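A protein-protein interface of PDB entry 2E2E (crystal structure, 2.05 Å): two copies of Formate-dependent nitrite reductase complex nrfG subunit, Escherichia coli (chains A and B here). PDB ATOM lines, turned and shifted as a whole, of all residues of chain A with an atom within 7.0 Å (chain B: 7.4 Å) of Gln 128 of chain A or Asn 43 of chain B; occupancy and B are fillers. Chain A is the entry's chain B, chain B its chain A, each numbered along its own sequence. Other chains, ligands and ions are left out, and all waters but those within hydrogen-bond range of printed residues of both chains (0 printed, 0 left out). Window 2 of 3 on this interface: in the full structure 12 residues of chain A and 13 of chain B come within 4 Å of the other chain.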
ATOM      1  N   HIS A  95       5.467 -11.167   4.843  1.00  0.00           N
ATOM      2  CA  HIS A  95       5.446 -10.982   6.290  1.00  0.00           C
ATOM      3  C   HIS A  95       5.328  -9.490   6.584  1.00  0.00           C
ATOM      4  O   HIS A  95       5.973  -8.693   5.914  1.00  0.00           O
ATOM      5  CB  HIS A  95       6.720 -11.559   6.945  1.00  0.00           C
ATOM      6  CG  HIS A  95       6.917 -13.031   6.707  1.00  0.00           C
ATOM      7  ND1 HIS A  95       6.623 -13.989   7.655  1.00  0.00           N
ATOM      8  CD2 HIS A  95       7.384 -13.706   5.626  1.00  0.00           C
ATOM      9  CE1 HIS A  95       6.879 -15.190   7.164  1.00  0.00           C
ATOM     10  NE2 HIS A  95       7.347 -15.046   5.935  1.00  0.00           N
ATOM     11  N   MET A  96       4.509  -9.116   7.581  1.00  0.00           N
ATOM     12  CA  MET A  96       4.351  -7.726   7.938  1.00  0.00           C
ATOM     13  C   MET A  96       5.673  -7.239   8.463  1.00  0.00           C
ATOM     14  O   MET A  96       6.514  -8.032   8.920  1.00  0.00           O
ATOM     15  CB  MET A  96       3.244  -7.501   8.992  1.00  0.00           C
ATOM     16  CG  MET A  96       2.757  -6.032   9.147  1.00  0.00           C
ATOM     17  SD  MET A  96       2.274  -5.124   7.646  1.00  0.00           S
ATOM     18  CE  MET A  96       0.765  -5.957   7.138  1.00  0.00           C
ATOM     19  N   THR A  97       5.830  -5.927   8.431  1.00  0.00           N
ATOM     20  CA  THR A  97       7.089  -5.285   8.619  1.00  0.00           C
ATOM     21  C   THR A  97       6.667  -3.900   9.092  1.00  0.00           C
ATOM     22  O   THR A  97       5.557  -3.452   8.783  1.00  0.00           O
ATOM     23  CB  THR A  97       7.828  -5.288   7.228  1.00  0.00           C
ATOM     24  OG1 THR A  97       9.028  -6.054   7.301  1.00  0.00           O
ATOM     25  CG2 THR A  97       8.122  -3.949   6.711  1.00  0.00           C
ATOM     26  N   ARG A 101       3.751  -1.583   7.487  1.00  0.00           N
ATOM     27  CA  ARG A 101       2.567  -1.140   8.191  1.00  0.00           C
ATOM     28  C   ARG A 101       2.425   0.367   8.113  1.00  0.00           C
ATOM     29  O   ARG A 101       1.301   0.866   8.083  1.00  0.00           O
ATOM     30  CB  ARG A 101       2.541  -1.594   9.640  1.00  0.00           C
ATOM     31  CG  ARG A 101       1.226  -1.292  10.307  1.00  0.00           C
ATOM     32  CD  ARG A 101       1.095  -1.983  11.638  1.00  0.00           C
ATOM     33  NE  ARG A 101       1.017  -3.432  11.467  1.00  0.00           N
ATOM     34  CZ  ARG A 101      -0.109  -4.113  11.257  1.00  0.00           C
ATOM     35  NH1 ARG A 101      -1.276  -3.477  11.186  1.00  0.00           N
ATOM     36  NH2 ARG A 101      -0.057  -5.431  11.122  1.00  0.00           N
ATOM     37  N   SER A 123      -5.476 -10.051   4.652  1.00  0.00           N
ATOM     38  CA  SER A 123      -4.713 -11.243   4.379  1.00  0.00           C
ATOM     39  C   SER A 123      -3.659 -11.468   5.436  1.00  0.00           C
ATOM     40  O   SER A 123      -3.356 -12.611   5.770  1.00  0.00           O
ATOM     41  CB  SER A 123      -4.021 -11.131   2.998  1.00  0.00           C
ATOM     42  OG  SER A 123      -4.886 -11.603   1.942  1.00  0.00           O
ATOM     43  N   ASP A 124      -3.070 -10.385   5.939  1.00  0.00           N
ATOM     44  CA  ASP A 124      -2.038 -10.544   6.923  1.00  0.00           C
ATOM     45  C   ASP A 124      -2.683 -10.947   8.262  1.00  0.00           C
ATOM     46  O   ASP A 124      -2.119 -11.754   8.989  1.00  0.00           O
ATOM     47  CB  ASP A 124      -1.256  -9.239   7.165  1.00  0.00           C
ATOM     48  CG  ASP A 124      -0.032  -9.474   8.056  1.00  0.00           C
ATOM     49  OD1 ASP A 124      -0.026  -8.993   9.196  1.00  0.00           O
ATOM     50  OD2 ASP A 124       0.882 -10.234   7.627  1.00  0.00           O
ATOM     51  N   ALA A 125      -3.802 -10.306   8.610  1.00  0.00           N
ATOM     52  CA  ALA A 125      -4.577 -10.718   9.813  1.00  0.00           C
ATOM     53  C   ALA A 125      -4.832 -12.236   9.746  1.00  0.00           C
ATOM     54  O   ALA A 125      -4.576 -12.964  10.696  1.00  0.00           O
ATOM     55  CB  ALA A 125      -5.865  -9.983   9.868  1.00  0.00           C
ATOM     56  N   PHE A 126      -5.304 -12.714   8.600  1.00  0.00           N
ATOM     57  CA  PHE A 126      -5.535 -14.144   8.380  1.00  0.00           C
ATOM     58  C   PHE A 126      -4.262 -14.949   8.663  1.00  0.00           C
ATOM     59  O   PHE A 126      -4.313 -16.006   9.275  1.00  0.00           O
ATOM     60  CB  PHE A 126      -5.961 -14.381   6.912  1.00  0.00           C
ATOM     61  CG  PHE A 126      -6.381 -15.812   6.589  1.00  0.00           C
ATOM     62  CD1 PHE A 126      -7.713 -16.126   6.379  1.00  0.00           C
ATOM     63  CD2 PHE A 126      -5.450 -16.804   6.427  1.00  0.00           C
ATOM     64  CE1 PHE A 126      -8.109 -17.431   6.027  1.00  0.00           C
ATOM     65  CE2 PHE A 126      -5.828 -18.102   6.094  1.00  0.00           C
ATOM     66  CZ  PHE A 126      -7.164 -18.419   5.895  1.00  0.00           C
ATOM     67  N   MET A 127      -3.117 -14.482   8.171  1.00  0.00           N
ATOM     68  CA  MET A 127      -1.894 -15.286   8.330  1.00  0.00           C
ATOM     69  C   MET A 127      -1.417 -15.281   9.807  1.00  0.00           C
ATOM     70  O   MET A 127      -0.745 -16.199  10.266  1.00  0.00           O
ATOM     71  CB  MET A 127      -0.804 -14.837   7.366  1.00  0.00           C
ATOM     72  CG  MET A 127      -1.029 -15.265   5.883  1.00  0.00           C
ATOM     73  SD  MET A 127      -1.425 -17.011   5.573  1.00  0.00           S
ATOM     74  CE  MET A 127       0.280 -17.609   5.672  1.00  0.00           C
ATOM     75  N   GLN A 128      -1.771 -14.239  10.539  1.00  0.00           N
ATOM     76  CA  GLN A 128      -1.460 -14.138  11.976  1.00  0.00           C
ATOM     77  C   GLN A 128      -2.567 -14.728  12.853  1.00  0.00           C
ATOM     78  O   GLN A 128      -2.529 -14.591  14.092  1.00  0.00           O
ATOM     79  CB  GLN A 128      -1.237 -12.671  12.359  1.00  0.00           C
ATOM     80  CG  GLN A 128      -0.055 -12.001  11.678  1.00  0.00           C
ATOM     81  CD  GLN A 128       0.436 -10.754  12.389  1.00  0.00           C
ATOM     82  OE1 GLN A 128       0.337 -10.633  13.631  1.00  0.00           O
ATOM     83  NE2 GLN A 128       0.997  -9.802  11.611  1.00  0.00           N
ATOM     84  N   ALA A 129      -3.569 -15.362  12.232  1.00  0.00           N
ATOM     85  CA  ALA A 129      -4.683 -16.006  12.967  1.00  0.00           C
ATOM     86  C   ALA A 129      -5.631 -15.043  13.641  1.00  0.00           C
ATOM     87  O   ALA A 129      -6.366 -15.451  14.594  1.00  0.00           O
ATOM     88  CB  ALA A 129      -4.179 -17.060  13.992  1.00  0.00           C
ATOM     89  N   ASN A 130      -5.615 -13.768  13.223  1.00  0.00           N
ATOM     90  CA  ASN A 130      -6.591 -12.835  13.758  1.00  0.00           C
ATOM     91  C   ASN A 130      -7.799 -12.849  12.861  1.00  0.00           C
ATOM     92  O   ASN A 130      -8.110 -11.859  12.227  1.00  0.00           O
ATOM     93  CB  ASN A 130      -6.040 -11.403  13.970  1.00  0.00           C
ATOM     94  CG  ASN A 130      -4.859 -11.358  14.935  1.00  0.00           C
ATOM     95  OD1 ASN A 130      -3.928 -10.556  14.765  1.00  0.00           O
ATOM     96  ND2 ASN A 130      -4.897 -12.195  15.973  1.00  0.00           N
ATOM     97  N   TYR A 131      -8.485 -13.986  12.803  1.00  0.00           N
ATOM     98  CA  TYR A 131      -9.566 -14.188  11.810  1.00  0.00           C
ATOM     99  C   TYR A 131     -10.692 -13.176  11.913  1.00  0.00           C
ATOM    100  O   TYR A 131     -11.258 -12.769  10.907  1.00  0.00           O
ATOM    101  CB  TYR A 131     -10.104 -15.611  11.883  1.00  0.00           C
ATOM    102  CG  TYR A 131      -9.010 -16.611  11.728  1.00  0.00           C
ATOM    103  CD1 TYR A 131      -8.628 -17.408  12.798  1.00  0.00           C
ATOM    104  CD2 TYR A 131      -8.345 -16.764  10.496  1.00  0.00           C
ATOM    105  CE1 TYR A 131      -7.582 -18.322  12.671  1.00  0.00           C
ATOM    106  CE2 TYR A 131      -7.316 -17.641  10.369  1.00  0.00           C
ATOM    107  CZ  TYR A 131      -6.953 -18.443  11.460  1.00  0.00           C
ATOM    108  OH  TYR A 131      -5.921 -19.354  11.338  1.00  0.00           O
ATOM    109  N   LYS B  36       4.576  -8.078  25.345  1.00  0.00           N
ATOM    110  CA  LYS B  36       4.010  -8.215  24.006  1.00  0.00           C
ATOM    111  C   LYS B  36       4.522  -9.442  23.228  1.00  0.00           C
ATOM    112  O   LYS B  36       3.847  -9.914  22.309  1.00  0.00           O
ATOM    113  CB  LYS B  36       4.240  -6.938  23.209  1.00  0.00           C
ATOM    114  CG  LYS B  36       3.362  -5.769  23.641  1.00  0.00           C
ATOM    115  CD  LYS B  36       2.359  -5.357  22.568  1.00  0.00           C
ATOM    116  CE  LYS B  36       3.056  -4.705  21.360  1.00  0.00           C
ATOM    117  NZ  LYS B  36       3.745  -3.410  21.670  1.00  0.00           N
ATOM    118  N   ILE B  37       5.712  -9.940  23.579  1.00  0.00           N
ATOM    119  CA  ILE B  37       6.240 -11.180  22.992  1.00  0.00           C
ATOM    120  C   ILE B  37       5.589 -12.400  23.650  1.00  0.00           C
ATOM    121  O   ILE B  37       5.282 -13.382  22.971  1.00  0.00           O
ATOM    122  CB  ILE B  37       7.789 -11.306  23.110  1.00  0.00           C
ATOM    123  CG1 ILE B  37       8.511 -10.176  22.362  1.00  0.00           C
ATOM    124  CG2 ILE B  37       8.257 -12.679  22.617  1.00  0.00           C
ATOM    125  CD1 ILE B  37       9.211 -10.582  21.075  1.00  0.00           C
ATOM    126  N   ASN B  40       2.153 -12.566  22.146  1.00  0.00           N
ATOM    127  CA  ASN B  40       2.202 -13.122  20.801  1.00  0.00           C
ATOM    128  C   ASN B  40       3.642 -13.469  20.436  1.00  0.00           C
ATOM    129  O   ASN B  40       4.463 -12.571  20.281  1.00  0.00           O
ATOM    130  CB  ASN B  40       1.611 -12.123  19.800  1.00  0.00           C
ATOM    131  CG  ASN B  40       1.258 -12.761  18.457  1.00  0.00           C
ATOM    132  OD1 ASN B  40       1.364 -13.982  18.274  1.00  0.00           O
ATOM    133  ND2 ASN B  40       0.834 -11.930  17.507  1.00  0.00           N
ATOM    134  N   PRO B  41       3.960 -14.772  20.336  1.00  0.00           N
ATOM    135  CA  PRO B  41       5.331 -15.231  20.127  1.00  0.00           C
ATOM    136  C   PRO B  41       5.768 -15.547  18.686  1.00  0.00           C
ATOM    137  O   PRO B  41       6.969 -15.686  18.444  1.00  0.00           O
ATOM    138  CB  PRO B  41       5.395 -16.505  20.988  1.00  0.00           C
ATOM    139  CG  PRO B  41       3.922 -16.924  21.203  1.00  0.00           C
ATOM    140  CD  PRO B  41       3.050 -15.914  20.494  1.00  0.00           C
ATOM    141  N   GLN B  42       4.834 -15.668  17.746  1.00  0.00           N
ATOM    142  CA  GLN B  42       5.188 -16.008  16.354  1.00  0.00           C
ATOM    143  C   GLN B  42       5.382 -14.796  15.441  1.00  0.00           C
ATOM    144  O   GLN B  42       5.606 -14.937  14.232  1.00  0.00           O
ATOM    145  CB  GLN B  42       4.177 -16.988  15.737  1.00  0.00           C
ATOM    146  CG  GLN B  42       4.732 -18.412  15.538  1.00  0.00           C
ATOM    147  CD  GLN B  42       4.954 -19.164  16.840  1.00  0.00           C
ATOM    148  OE1 GLN B  42       4.200 -19.000  17.805  1.00  0.00           O
ATOM    149  NE2 GLN B  42       5.986 -20.006  16.870  1.00  0.00           N
ATOM    150  N   ASN B  43       5.308 -13.609  16.026  1.00  0.00           N
ATOM    151  CA  ASN B  43       5.483 -12.379  15.265  1.00  0.00           C
ATOM    152  C   ASN B  43       6.965 -12.012  15.039  1.00  0.00           C
ATOM    153  O   ASN B  43       7.702 -11.720  15.979  1.00  0.00           O
ATOM    154  CB  ASN B  43       4.674 -11.234  15.904  1.00  0.00           C
ATOM    155  CG  ASN B  43       4.530 -10.027  14.985  1.00  0.00           C
ATOM    156  OD1 ASN B  43       5.408  -9.734  14.169  1.00  0.00           O
ATOM    157  ND2 ASN B  43       3.426  -9.307  15.133  1.00  0.00           N
ATOM    158  N   SER B  44       7.375 -12.056  13.772  1.00  0.00           N
ATOM    159  CA  SER B  44       8.713 -11.662  13.326  1.00  0.00           C
ATOM    160  C   SER B  44       9.189 -10.292  13.841  1.00  0.00           C
ATOM    161  O   SER B  44      10.237 -10.181  14.489  1.00  0.00           O
ATOM    162  CB  SER B  44       8.747 -11.641  11.795  1.00  0.00           C
ATOM    163  OG  SER B  44       9.106 -12.902  11.265  1.00  0.00           O
ATOM    164  N   GLU B  45       8.417  -9.252  13.545  1.00  0.00           N
ATOM    165  CA  GLU B  45       8.861  -7.882  13.812  1.00  0.00           C
ATOM    166  C   GLU B  45       8.931  -7.572  15.326  1.00  0.00           C
ATOM    167  O   GLU B  45       9.655  -6.670  15.743  1.00  0.00           O
ATOM    168  CB  GLU B  45       7.994  -6.876  13.012  1.00  0.00           C
ATOM    169  CG  GLU B  45       8.557  -5.471  12.825  1.00  0.00           C
ATOM    170  CD  GLU B  45       9.580  -5.315  11.674  1.00  0.00           C
ATOM    171  OE1 GLU B  45       9.844  -4.169  11.296  1.00  0.00           O
ATOM    172  OE2 GLU B  45      10.152  -6.292  11.157  1.00  0.00           O
ATOM    173  N   GLN B  46       8.212  -8.338  16.141  1.00  0.00           N
ATOM    174  CA  GLN B  46       8.270  -8.184  17.601  1.00  0.00           C
ATOM    175  C   GLN B  46       9.630  -8.606  18.176  1.00  0.00           C
ATOM    176  O   GLN B  46      10.140  -7.987  19.111  1.00  0.00           O
ATOM    177  CB  GLN B  46       7.175  -9.009  18.264  1.00  0.00           C
ATOM    178  CG  GLN B  46       5.786  -8.466  18.107  1.00  0.00           C
ATOM    179  CD  GLN B  46       5.318  -7.693  19.337  1.00  0.00           C
ATOM    180  OE1 GLN B  46       5.573  -6.483  19.471  1.00  0.00           O
ATOM    181  NE2 GLN B  46       4.613  -8.386  20.231  1.00  0.00           N
ATOM    182  N   TRP B  47      10.197  -9.677  17.625  1.00  0.00           N
ATOM    183  CA  TRP B  47      11.520 -10.144  18.038  1.00  0.00           C
ATOM    184  C   TRP B  47      12.615  -9.218  17.501  1.00  0.00           C
ATOM    185  O   TRP B  47      13.691  -9.074  18.101  1.00  0.00           O
ATOM    186  CB  TRP B  47      11.752 -11.554  17.536  1.00  0.00           C
ATOM    187  CG  TRP B  47      11.010 -12.594  18.318  1.00  0.00           C
ATOM    188  CD1 TRP B  47       9.790 -13.142  18.015  1.00  0.00           C
ATOM    189  CD2 TRP B  47      11.421 -13.182  19.547  1.00  0.00           C
ATOM    190  NE1 TRP B  47       9.426 -14.053  18.978  1.00  0.00           N
ATOM    191  CE2 TRP B  47      10.412 -14.103  19.929  1.00  0.00           C
ATOM    192  CE3 TRP B  47      12.559 -13.045  20.358  1.00  0.00           C
ATOM    193  CZ2 TRP B  47      10.504 -14.880  21.087  1.00  0.00           C
ATOM    194  CZ3 TRP B  47      12.653 -13.820  21.507  1.00  0.00           C
ATOM    195  CH2 TRP B  47      11.626 -14.722  21.863  1.00  0.00           C
ATOM    196  N   ALA B  48      12.336  -8.601  16.358  1.00  0.00           N
ATOM    197  CA  ALA B  48      13.289  -7.701  15.719  1.00  0.00           C
ATOM    198  C   ALA B  48      13.405  -6.440  16.562  1.00  0.00           C
ATOM    199  O   ALA B  48      14.493  -5.919  16.739  1.00  0.00           O
ATOM    200  CB  ALA B  48      12.847  -7.367  14.304  1.00  0.00           C
ATOM    201  N   GLN B  69      15.835 -15.287  16.340  1.00  0.00           N
ATOM    202  CA  GLN B  69      14.466 -15.745  16.435  1.00  0.00           C
ATOM    203  C   GLN B  69      13.575 -15.072  15.384  1.00  0.00           C
ATOM    204  O   GLN B  69      12.820 -15.755  14.680  1.00  0.00           O
ATOM    205  CB  GLN B  69      13.923 -15.515  17.845  1.00  0.00           C
ATOM    206  CG  GLN B  69      12.505 -16.027  18.056  1.00  0.00           C
ATOM    207  CD  GLN B  69      12.394 -17.544  18.148  1.00  0.00           C
ATOM    208  OE1 GLN B  69      13.280 -18.209  18.639  1.00  0.00           O
ATOM    209  NE2 GLN B  69      11.273 -18.083  17.684  1.00  0.00           N
ATOM    210  N   ALA B  70      13.663 -13.740  15.285  1.00  0.00           N
ATOM    211  CA  ALA B  70      12.984 -12.997  14.232  1.00  0.00           C
ATOM    212  C   ALA B  70      13.180 -13.672  12.875  1.00  0.00           C
ATOM    213  O   ALA B  70      12.216 -13.902  12.152  1.00  0.00           O
ATOM    214  CB  ALA B  70      13.479 -11.540  14.194  1.00  0.00           C
ATOM    215  N   LEU B  73      11.600 -17.230  12.201  1.00  0.00           N
ATOM    216  CA  LEU B  73      10.195 -17.059  11.907  1.00  0.00           C
ATOM    217  C   LEU B  73       9.905 -16.523  10.496  1.00  0.00           C
ATOM    218  O   LEU B  73       8.968 -16.986   9.841  1.00  0.00           O
ATOM    219  CB  LEU B  73       9.575 -16.128  12.956  1.00  0.00           C
ATOM    220  CG  LEU B  73       9.462 -16.590  14.408  1.00  0.00           C
ATOM    221  CD1 LEU B  73       9.181 -15.426  15.326  1.00  0.00           C
ATOM    222  CD2 LEU B  73       8.373 -17.681  14.572  1.00  0.00           C
ATOM    223  N   ARG B  74      10.689 -15.544  10.039  1.00  0.00           N
ATOM    224  CA  ARG B  74      10.403 -14.826   8.792  1.00  0.00           C
ATOM    225  C   ARG B  74      10.945 -15.518   7.553  1.00  0.00           C
ATOM    226  O   ARG B  74      10.428 -15.322   6.433  1.00  0.00           O
ATOM    227  CB  ARG B  74      10.968 -13.391   8.839  1.00  0.00           C
ATOM    228  CG  ARG B  74      10.296 -12.458   7.832  1.00  0.00           C
ATOM    229  CD  ARG B  74      10.673 -10.991   7.980  1.00  0.00           C
ATOM    230  NE  ARG B  74      10.039 -10.377   9.138  1.00  0.00           N
ATOM    231  CZ  ARG B  74      10.315  -9.157   9.590  1.00  0.00           C
ATOM    232  NH1 ARG B  74      11.200  -8.377   8.976  1.00  0.00           N
ATOM    233  NH2 ARG B  74       9.684  -8.703  10.655  1.00  0.00           N
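O of Arg 74 of chain B is in hydrogen-bond range of NE2 of His 95 of chain A, 3.1 Å away.
The backbone NH of Arg 74 of chain B sits close to the side-chain hydroxyl of Ser 44 of chain B (3.3 Å). N of Glu 45 of chain B sits at hydrogen-bond distance from OD1 of Asn 43 of chain B (3.1 Å). The side-chain carboxylate of Glu 45 of chain B lies within salt-bridge range of the guanidinium group of Arg 74 of chain B (2.5 Å). The side-chain amide nitrogen (NE2) of Gln 128 of chain A sits at hydrogen-bond distance from the side-chain carboxylate (OD1) of Asp 124 of chain A (2.7 Å).
Among the printed residues, merely in contact across the chains: His 95 of chain A with Leu 73 of chain B, Met 96 of chain A with Arg 74 of chain B, Thr 97 of chain A with Glu 45 of chain B, Thr 97 of chain A with Arg 74 of chain B and Gln 128 of chain A with Asn 43 of chain B.
Asn 43 of chain B touches just one residue of chain A: Gln 128. Printed residues of chain A within 4 Å of Arg 74 of chain B: His 95 (3.1 Å), Met 96 (3.7 Å) and Thr 97 (3.6 Å). Of the printed residues of chain A, Glu 45 of chain B touches Thr 97. Of the printed residues of chain B, Thr 97 of chain A touches Glu 45 (3.9 Å) and Arg 74 (3.6 Å). Printed residues of chain A within 4 Å of Leu 73 of chain B: His 95.
Of the 15 printed residues of chain B, 4 touch a printed residue of chain A. Printed residues of chain B that touch a printed residue of chain A: Asn 43, Glu 45, Leu 73 and Arg 74. Of the 13 printed residues of chain A, 4 touch a printed residue of chain B. Hydrophobic or aromatic side chains of chain A that line the printed part of chain B: His 95. Among the printed residues, 6 pairs touch across the chains. Among the printed residues, no Asp or Glu carboxylate lies within 4 Å of a Lys or Arg side-chain nitrogen of the other chain.
No position is printed for both chains. Of the 6 pairs that touch across the chains among the printed residues, none has its exchanged pair printed and touching as well.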
